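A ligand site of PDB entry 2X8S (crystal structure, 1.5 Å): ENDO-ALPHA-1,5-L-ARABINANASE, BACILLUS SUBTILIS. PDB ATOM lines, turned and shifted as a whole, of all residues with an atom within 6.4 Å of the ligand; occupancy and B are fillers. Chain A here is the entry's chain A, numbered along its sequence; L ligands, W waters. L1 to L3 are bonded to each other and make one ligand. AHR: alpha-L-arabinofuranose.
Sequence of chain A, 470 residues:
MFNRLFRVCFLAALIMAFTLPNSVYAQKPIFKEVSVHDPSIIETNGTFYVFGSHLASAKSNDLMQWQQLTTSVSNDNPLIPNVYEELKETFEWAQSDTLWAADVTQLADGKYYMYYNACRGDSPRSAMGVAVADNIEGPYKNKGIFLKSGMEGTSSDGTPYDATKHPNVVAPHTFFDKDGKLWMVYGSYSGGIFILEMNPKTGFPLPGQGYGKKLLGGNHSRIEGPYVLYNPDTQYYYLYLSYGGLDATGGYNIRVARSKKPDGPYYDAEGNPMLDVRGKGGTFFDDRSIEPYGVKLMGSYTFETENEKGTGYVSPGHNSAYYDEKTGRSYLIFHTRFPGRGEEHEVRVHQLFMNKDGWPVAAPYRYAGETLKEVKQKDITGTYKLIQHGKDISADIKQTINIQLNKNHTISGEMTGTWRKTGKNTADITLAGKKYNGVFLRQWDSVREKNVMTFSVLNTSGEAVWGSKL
Water W2 lies within hydrogen-bond range of an oxygen (O3) of AHR L2 (2.7 Å), the side-chain hydroxyl of Ser 188 (2.8 Å) and the side-chain amide nitrogen of Asn 168 (3.0 Å).
Water W1 lies within hydrogen-bond range of the side-chain carboxylate (OE2) of Glu 224 (2.8 Å), the side-chain hydroxyl (OH) of Tyr 189 (2.9 Å), an oxygen (O5) of AHR L3 (2.9 Å) and the backbone NH (N) of Leu 246 (3.1 Å).
O3 of AHR L2 sits at hydrogen-bond distance from O of Ser 188.
ND2 of Asn 168 lies within hydrogen-bond range of O3 of AHR L2, 3.4 Å away.
The side-chain hydroxyl of Tyr 189 lies within hydrogen-bond range of an oxygen (O3) of AHR L3 (3.3 Å).
An oxygen (O5) of AHR L3 is in hydrogen-bond range of the side-chain carboxylate of Glu 224, at 2.7 Å.
OG of Ser 190 is in hydrogen-bond range of O3 of AHR L2 (2.8 Å).
N of Ser 190 lies within hydrogen-bond range of O2 of AHR L2.
O2 of AHR L2 is in hydrogen-bond range of ND1 of His 220, 2.7 Å away.
The backbone NH (N) of Phe 285 lies within hydrogen-bond range of the backbone carbonyl oxygen (O) of His 220 (2.9 Å).
SG of Cys 119 sits at hydrogen-bond distance from O of Ser 123 (3.2 Å).
The side-chain hydroxyl of Tyr 189 lies within hydrogen-bond range of the backbone carbonyl oxygen of Gly 244 (3.1 Å).
O of Ser 190 sits at hydrogen-bond distance from N of His 220 (2.9 Å).
The side-chain carboxylate of Glu 224 is in hydrogen-bond range of the side-chain hydroxyl of Ser 188 (2.6 Å).
ND2 of Asn 168 sits at hydrogen-bond distance from SG of Cys 119, at 3.6 Å.
The side-chain carboxylate (OE2) of Glu 224 is in hydrogen-bond range of the side-chain hydroxyl (OH) of Tyr 252 (2.6 Å).
N of Gly 121 lies close to SG of Cys 119.
Residues that only touch the ligand: Phe 284, Trp 100, Pro 124, Ser 123, Leu 246, Asp 122 and Gly 121.
Hydrophobic or aromatic side chains that line the ligand: Trp 100, Pro 124, Tyr 189, His 220, Leu 246 and Phe 284.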
ATOM      1  N   TRP A 100     -36.146  25.542  19.546  1.00  0.00           N
ATOM      2  CA  TRP A 100     -34.966  24.836  19.056  1.00  0.00           C
ATOM      3  C   TRP A 100     -34.975  24.767  17.519  1.00  0.00           C
ATOM      4  O   TRP A 100     -35.653  25.555  16.862  1.00  0.00           O
ATOM      5  CB  TRP A 100     -34.832  23.485  19.754  1.00  0.00           C
ATOM      6  CG  TRP A 100     -34.186  23.625  21.110  1.00  0.00           C
ATOM      7  CD1 TRP A 100     -34.106  24.766  21.872  1.00  0.00           C
ATOM      8  CD2 TRP A 100     -33.524  22.604  21.873  1.00  0.00           C
ATOM      9  NE1 TRP A 100     -33.430  24.506  23.045  1.00  0.00           N
ATOM     10  CE2 TRP A 100     -33.065  23.188  23.068  1.00  0.00           C
ATOM     11  CE3 TRP A 100     -33.271  21.248  21.640  1.00  0.00           C
ATOM     12  CZ2 TRP A 100     -32.366  22.473  24.039  1.00  0.00           C
ATOM     13  CZ3 TRP A 100     -32.578  20.525  22.611  1.00  0.00           C
ATOM     14  CH2 TRP A 100     -32.138  21.146  23.787  1.00  0.00           C
ATOM     15  N   CYS A 119     -37.475  22.717  23.865  1.00  0.00           N
ATOM     16  CA  CYS A 119     -36.980  21.764  24.852  1.00  0.00           C
ATOM     17  C   CYS A 119     -36.510  22.497  26.103  1.00  0.00           C
ATOM     18  O   CYS A 119     -35.904  23.574  26.028  1.00  0.00           O
ATOM     19  CB  CYS A 119     -35.817  20.977  24.233  1.00  0.00           C
ATOM     20  SG  CYS A 119     -34.992  19.836  25.353  1.00  0.00           S
ATOM     21  N   GLY A 121     -34.134  21.796  28.009  1.00  0.00           N
ATOM     22  CA  GLY A 121     -32.705  21.939  27.794  1.00  0.00           C
ATOM     23  C   GLY A 121     -31.842  21.092  28.703  1.00  0.00           C
ATOM     24  O   GLY A 121     -30.685  20.806  28.376  1.00  0.00           O
ATOM     25  N   ASP A 122     -32.393  20.681  29.847  1.00  0.00           N
ATOM     26  CA  ASP A 122     -31.667  19.851  30.796  1.00  0.00           C
ATOM     27  C   ASP A 122     -32.178  18.425  30.757  1.00  0.00           C
ATOM     28  O   ASP A 122     -31.716  17.562  31.510  1.00  0.00           O
ATOM     29  CB  ASP A 122     -31.805  20.421  32.214  1.00  0.00           C
ATOM     30  CG  ASP A 122     -33.254  20.513  32.665  1.00  0.00           C
ATOM     31  OD1 ASP A 122     -33.485  20.814  33.858  1.00  0.00           O
ATOM     32  OD2 ASP A 122     -34.174  20.288  31.836  1.00  0.00           O
ATOM     33  N   SER A 123     -33.133  18.177  29.871  1.00  0.00           N
ATOM     34  CA  SER A 123     -33.869  16.925  29.816  1.00  0.00           C
ATOM     35  C   SER A 123     -34.707  17.019  28.556  1.00  0.00           C
ATOM     36  O   SER A 123     -34.872  18.122  28.024  1.00  0.00           O
ATOM     37  CB  SER A 123     -34.786  16.795  31.034  1.00  0.00           C
ATOM     38  OG  SER A 123     -35.697  17.887  31.074  1.00  0.00           O
ATOM     39  N   PRO A 124     -35.212  15.879  28.053  1.00  0.00           N
ATOM     40  CA  PRO A 124     -35.978  15.913  26.794  1.00  0.00           C
ATOM     41  C   PRO A 124     -37.442  16.275  27.026  1.00  0.00           C
ATOM     42  O   PRO A 124     -38.344  15.644  26.473  1.00  0.00           O
ATOM     43  CB  PRO A 124     -35.846  14.477  26.277  1.00  0.00           C
ATOM     44  CG  PRO A 124     -35.736  13.643  27.538  1.00  0.00           C
ATOM     45  CD  PRO A 124     -34.997  14.503  28.544  1.00  0.00           C
ATOM     46  N   ALA A 163     -36.393   7.958  28.129  1.00  0.00           N
ATOM     47  CA  ALA A 163     -35.415   8.686  27.329  1.00  0.00           C
ATOM     48  C   ALA A 163     -34.215   7.870  26.856  1.00  0.00           C
ATOM     49  O   ALA A 163     -33.450   8.356  26.048  1.00  0.00           O
ATOM     50  CB  ALA A 163     -34.936   9.945  28.069  1.00  0.00           C
ATOM     51  N   ASN A 168     -35.949  12.639  21.916  1.00  0.00           N
ATOM     52  CA  ASN A 168     -36.295  13.994  22.254  1.00  0.00           C
ATOM     53  C   ASN A 168     -36.930  14.543  20.975  1.00  0.00           C
ATOM     54  O   ASN A 168     -36.331  14.449  19.899  1.00  0.00           O
ATOM     55  CB  ASN A 168     -35.020  14.766  22.582  1.00  0.00           C
ATOM     56  CG  ASN A 168     -35.301  16.118  23.201  1.00  0.00           C
ATOM     57  OD1 ASN A 168     -36.459  16.442  23.493  1.00  0.00           O
ATOM     58  ND2 ASN A 168     -34.256  16.904  23.417  1.00  0.00           N
ATOM     59  N   SER A 188     -32.610  14.219  18.931  1.00  0.00           N
ATOM     60  CA  SER A 188     -31.384  14.727  19.537  1.00  0.00           C
ATOM     61  C   SER A 188     -31.106  13.961  20.806  1.00  0.00           C
ATOM     62  O   SER A 188     -31.924  13.977  21.730  1.00  0.00           O
ATOM     63  CB  SER A 188     -31.506  16.210  19.876  1.00  0.00           C
ATOM     64  OG  SER A 188     -30.387  16.616  20.656  1.00  0.00           O
ATOM     65  N   TYR A 189     -29.938  13.331  20.880  1.00  0.00           N
ATOM     66  CA  TYR A 189     -29.530  12.599  22.080  1.00  0.00           C
ATOM     67  C   TYR A 189     -30.659  11.634  22.505  1.00  0.00           C
ATOM     68  O   TYR A 189     -31.276  11.001  21.653  1.00  0.00           O
ATOM     69  CB  TYR A 189     -29.161  13.571  23.211  1.00  0.00           C
ATOM     70  CG  TYR A 189     -27.908  14.435  23.020  1.00  0.00           C
ATOM     71  CD1 TYR A 189     -27.565  14.976  21.787  1.00  0.00           C
ATOM     72  CD2 TYR A 189     -27.087  14.719  24.110  1.00  0.00           C
ATOM     73  CE1 TYR A 189     -26.419  15.777  21.642  1.00  0.00           C
ATOM     74  CE2 TYR A 189     -25.962  15.509  23.972  1.00  0.00           C
ATOM     75  CZ  TYR A 189     -25.638  16.039  22.736  1.00  0.00           C
ATOM     76  OH  TYR A 189     -24.501  16.821  22.622  1.00  0.00           O
ATOM     77  N   SER A 190     -30.927  11.523  23.808  1.00  0.00           N
ATOM     78  CA  SER A 190     -31.973  10.633  24.293  1.00  0.00           C
ATOM     79  C   SER A 190     -31.954   9.254  23.611  1.00  0.00           C
ATOM     80  O   SER A 190     -30.910   8.603  23.548  1.00  0.00           O
ATOM     81  CB  SER A 190     -33.348  11.307  24.179  1.00  0.00           C
ATOM     82  OG  SER A 190     -33.417  12.436  25.044  1.00  0.00           O
ATOM     83  N   GLY A 191     -33.091   8.804  23.090  1.00  0.00           N
ATOM     84  CA  GLY A 191     -33.195   7.443  22.575  1.00  0.00           C
ATOM     85  C   GLY A 191     -32.819   7.258  21.112  1.00  0.00           C
ATOM     86  O   GLY A 191     -32.844   6.132  20.618  1.00  0.00           O
ATOM     87  N   ASN A 219     -29.596   5.342  24.490  1.00  0.00           N
ATOM     88  CA  ASN A 219     -28.790   5.525  25.691  1.00  0.00           C
ATOM     89  C   ASN A 219     -28.065   6.868  25.744  1.00  0.00           C
ATOM     90  O   ASN A 219     -26.908   6.945  26.179  1.00  0.00           O
ATOM     91  CB  ASN A 219     -27.782   4.373  25.864  1.00  0.00           C
ATOM     92  CG  ASN A 219     -28.455   3.025  26.007  1.00  0.00           C
ATOM     93  OD1 ASN A 219     -29.627   3.011  26.623  1.00  0.00           O
ATOM     94  ND2 ASN A 219     -27.919   2.003  25.580  1.00  0.00           N
ATOM     95  N   HIS A 220     -28.718   7.923  25.278  1.00  0.00           N
ATOM     96  CA  HIS A 220     -28.204   9.272  25.430  1.00  0.00           C
ATOM     97  C   HIS A 220     -26.883   9.431  24.686  1.00  0.00           C
ATOM     98  O   HIS A 220     -25.928  10.015  25.204  1.00  0.00           O
ATOM     99  CB  HIS A 220     -28.044   9.628  26.905  1.00  0.00           C
ATOM    100  CG  HIS A 220     -29.321   9.534  27.692  1.00  0.00           C
ATOM    101  ND1 HIS A 220     -30.299  10.506  27.639  1.00  0.00           N
ATOM    102  CD2 HIS A 220     -29.763   8.600  28.568  1.00  0.00           C
ATOM    103  CE1 HIS A 220     -31.293  10.174  28.442  1.00  0.00           C
ATOM    104  NE2 HIS A 220     -30.993   9.016  29.019  1.00  0.00           N
ATOM    105  N   SER A 221     -26.837   8.918  23.458  1.00  0.00           N
ATOM    106  CA  SER A 221     -25.720   9.146  22.549  1.00  0.00           C
ATOM    107  C   SER A 221     -25.700  10.592  22.100  1.00  0.00           C
ATOM    108  O   SER A 221     -26.762  11.169  21.838  1.00  0.00           O
ATOM    109  CB  SER A 221     -25.850   8.271  21.294  1.00  0.00           C
ATOM    110  OG  SER A 221     -25.899   6.896  21.626  1.00  0.00           O
ATOM    111  N   ARG A 222     -24.510  11.183  21.958  1.00  0.00           N
ATOM    112  CA  ARG A 222     -24.438  12.548  21.437  1.00  0.00           C
ATOM    113  C   ARG A 222     -24.508  12.556  19.908  1.00  0.00           C
ATOM    114  O   ARG A 222     -23.523  12.734  19.203  1.00  0.00           O
ATOM    115  CB  ARG A 222     -23.187  13.271  21.951  1.00  0.00           C
ATOM    116  CG  ARG A 222     -23.078  13.249  23.489  1.00  0.00           C
ATOM    117  CD  ARG A 222     -22.287  14.450  24.005  1.00  0.00           C
ATOM    118  NE  ARG A 222     -20.879  14.333  23.682  1.00  0.00           N
ATOM    119  CZ  ARG A 222     -20.011  15.324  23.826  1.00  0.00           C
ATOM    120  NH1 ARG A 222     -18.731  15.123  23.536  1.00  0.00           N
ATOM    121  NH2 ARG A 222     -20.422  16.515  24.261  1.00  0.00           N
ATOM    122  N   GLU A 224     -27.324  14.150  16.942  1.00  0.00           N
ATOM    123  CA  GLU A 224     -28.520  14.970  16.767  1.00  0.00           C
ATOM    124  C   GLU A 224     -28.571  15.623  15.396  1.00  0.00           C
ATOM    125  O   GLU A 224     -27.592  15.578  14.622  1.00  0.00           O
ATOM    126  CB  GLU A 224     -28.592  16.046  17.864  1.00  0.00           C
ATOM    127  CG  GLU A 224     -27.519  17.138  17.711  1.00  0.00           C
ATOM    128  CD  GLU A 224     -27.494  18.111  18.871  1.00  0.00           C
ATOM    129  OE1 GLU A 224     -28.387  18.034  19.749  1.00  0.00           O
ATOM    130  OE2 GLU A 224     -26.580  18.966  18.928  1.00  0.00           O
ATOM    131  N   GLY A 244     -21.282  14.445  18.839  1.00  0.00           N
ATOM    132  CA  GLY A 244     -20.619  15.247  19.846  1.00  0.00           C
ATOM    133  C   GLY A 244     -21.447  16.403  20.350  1.00  0.00           C
ATOM    134  O   GLY A 244     -22.660  16.490  20.101  1.00  0.00           O
ATOM    135  N   GLY A 245     -20.781  17.285  21.060  1.00  0.00           N
ATOM    136  CA  GLY A 245     -21.449  18.466  21.544  1.00  0.00           C
ATOM    137  C   GLY A 245     -21.177  19.740  20.767  1.00  0.00           C
ATOM    138  O   GLY A 245     -20.156  19.925  20.255  1.00  0.00           O
ATOM    139  N   LEU A 246     -22.188  20.590  20.711  1.00  0.00           N
ATOM    140  CA  LEU A 246     -22.106  21.799  19.922  1.00  0.00           C
ATOM    141  C   LEU A 246     -21.115  22.880  20.370  1.00  0.00           C
ATOM    142  O   LEU A 246     -20.740  23.650  19.601  1.00  0.00           O
ATOM    143  CB  LEU A 246     -23.475  22.446  19.771  1.00  0.00           C
ATOM    144  CG  LEU A 246     -24.109  22.918  21.084  1.00  0.00           C
ATOM    145  CD1 LEU A 246     -23.814  24.364  21.311  1.00  0.00           C
ATOM    146  CD2 LEU A 246     -25.602  22.726  21.146  1.00  0.00           C
ATOM    147  N   TYR A 252     -17.974  18.689  18.167  1.00  0.00           N
ATOM    148  CA  TYR A 252     -19.032  18.550  17.164  1.00  0.00           C
ATOM    149  C   TYR A 252     -18.387  18.252  15.834  1.00  0.00           C
ATOM    150  O   TYR A 252     -17.413  18.838  15.481  1.00  0.00           O
ATOM    151  CB  TYR A 252     -19.802  19.856  17.004  1.00  0.00           C
ATOM    152  CG  TYR A 252     -21.338  19.854  16.892  1.00  0.00           C
ATOM    153  CD1 TYR A 252     -22.080  18.935  17.548  1.00  0.00           C
ATOM    154  CD2 TYR A 252     -21.995  20.822  16.198  1.00  0.00           C
ATOM    155  CE1 TYR A 252     -23.407  18.996  17.545  1.00  0.00           C
ATOM    156  CE2 TYR A 252     -23.349  20.877  16.190  1.00  0.00           C
ATOM    157  CZ  TYR A 252     -24.048  19.953  16.857  1.00  0.00           C
ATOM    158  OH  TYR A 252     -25.407  19.986  16.860  1.00  0.00           O
ATOM    159  N   PHE A 284     -24.324   7.618  29.896  1.00  0.00           N
ATOM    160  CA  PHE A 284     -24.729   8.873  29.265  1.00  0.00           C
ATOM    161  C   PHE A 284     -23.579   9.463  28.445  1.00  0.00           C
ATOM    162  O   PHE A 284     -22.439   9.526  28.908  1.00  0.00           O
ATOM    163  CB  PHE A 284     -25.124   9.915  30.317  1.00  0.00           C
ATOM    164  CG  PHE A 284     -26.429   9.627  31.006  1.00  0.00           C
ATOM    165  CD1 PHE A 284     -26.534   8.609  31.934  1.00  0.00           C
ATOM    166  CD2 PHE A 284     -27.540  10.405  30.742  1.00  0.00           C
ATOM    167  CE1 PHE A 284     -27.732   8.347  32.572  1.00  0.00           C
ATOM    168  CE2 PHE A 284     -28.749  10.162  31.375  1.00  0.00           C
ATOM    169  CZ  PHE A 284     -28.838   9.122  32.288  1.00  0.00           C
ATOM    170  N   PHE A 285     -23.899   9.918  27.234  1.00  0.00           N
ATOM    171  CA  PHE A 285     -22.935  10.609  26.394  1.00  0.00           C
ATOM    172  C   PHE A 285     -21.677   9.770  26.183  1.00  0.00           C
ATOM    173  O   PHE A 285     -20.559  10.282  26.230  1.00  0.00           O
ATOM    174  CB  PHE A 285     -22.593  11.976  27.001  1.00  0.00           C
ATOM    175  CG  PHE A 285     -23.778  12.682  27.592  1.00  0.00           C
ATOM    176  CD1 PHE A 285     -24.957  12.820  26.882  1.00  0.00           C
ATOM    177  CD2 PHE A 285     -23.713  13.216  28.873  1.00  0.00           C
ATOM    178  CE1 PHE A 285     -26.055  13.470  27.427  1.00  0.00           C
ATOM    179  CE2 PHE A 285     -24.814  13.866  29.427  1.00  0.00           C
ATOM    180  CZ  PHE A 285     -25.973  13.991  28.702  1.00  0.00           C
HETATM  181  O5  AHR L   1     -31.322  13.796  29.267  1.00  0.00           O
HETATM  182  C5  AHR L   1     -31.015  14.144  30.518  1.00  0.00           C
HETATM  183  C4  AHR L   1     -31.868  13.256  31.414  1.00  0.00           C
HETATM  184  O4  AHR L   1     -33.223  13.722  31.390  1.00  0.00           O
HETATM  185  C3  AHR L   1     -31.421  13.251  32.858  1.00  0.00           C
HETATM  186  O3  AHR L   1     -30.891  11.969  33.211  1.00  0.00           O
HETATM  187  C2  AHR L   1     -32.665  13.532  33.682  1.00  0.00           C
HETATM  188  O2  AHR L   1     -32.510  14.757  34.388  1.00  0.00           O
HETATM  189  C1  AHR L   1     -33.805  13.641  32.684  1.00  0.00           C
HETATM  190  O1  AHR L   1     -34.613  12.459  32.739  1.00  0.00           O
HETATM  191  O5  AHR L   2     -29.669  17.547  26.250  1.00  0.00           O
HETATM  192  C5  AHR L   2     -30.961  17.514  26.553  1.00  0.00           C
HETATM  193  C4  AHR L   2     -31.403  16.111  26.969  1.00  0.00           C
HETATM  194  O4  AHR L   2     -30.743  15.753  28.180  1.00  0.00           O
HETATM  195  C3  AHR L   2     -31.009  15.021  25.974  1.00  0.00           C
HETATM  196  O3  AHR L   2     -31.965  14.839  24.905  1.00  0.00           O
HETATM  197  C2  AHR L   2     -30.917  13.800  26.863  1.00  0.00           C
HETATM  198  O2  AHR L   2     -29.997  12.836  26.326  1.00  0.00           O
HETATM  199  C1  AHR L   2     -30.510  14.342  28.226  1.00  0.00           C
HETATM  200  O5  AHR L   3     -27.729  19.974  21.551  1.00  0.00           O
HETATM  201  C5  AHR L   3     -28.802  20.187  22.398  1.00  0.00           C
HETATM  202  C4  AHR L   3     -28.484  19.217  23.524  1.00  0.00           C
HETATM  203  O4  AHR L   3     -29.620  18.944  24.351  1.00  0.00           O
HETATM  204  C3  AHR L   3     -27.391  19.708  24.463  1.00  0.00           C
HETATM  205  O3  AHR L   3     -26.081  19.434  23.941  1.00  0.00           O
HETATM  206  C2  AHR L   3     -27.697  18.925  25.732  1.00  0.00           C
HETATM  207  O2  AHR L   3     -27.229  19.600  26.897  1.00  0.00           O
HETATM  208  C1  AHR L   3     -29.219  18.803  25.719  1.00  0.00           C
HETATM  209  O   HOH W   1     -24.903  19.267  21.176  1.00  0.00           O
HETATM  210  O   HOH W   2     -31.240  16.883  23.262  1.00  0.00           O
HETATM  211  O   HOH W   3     -28.239  17.157  28.967  1.00  0.00           O
HETATM  212  O   HOH W   4     -24.174  18.339  27.047  1.00  0.00           O
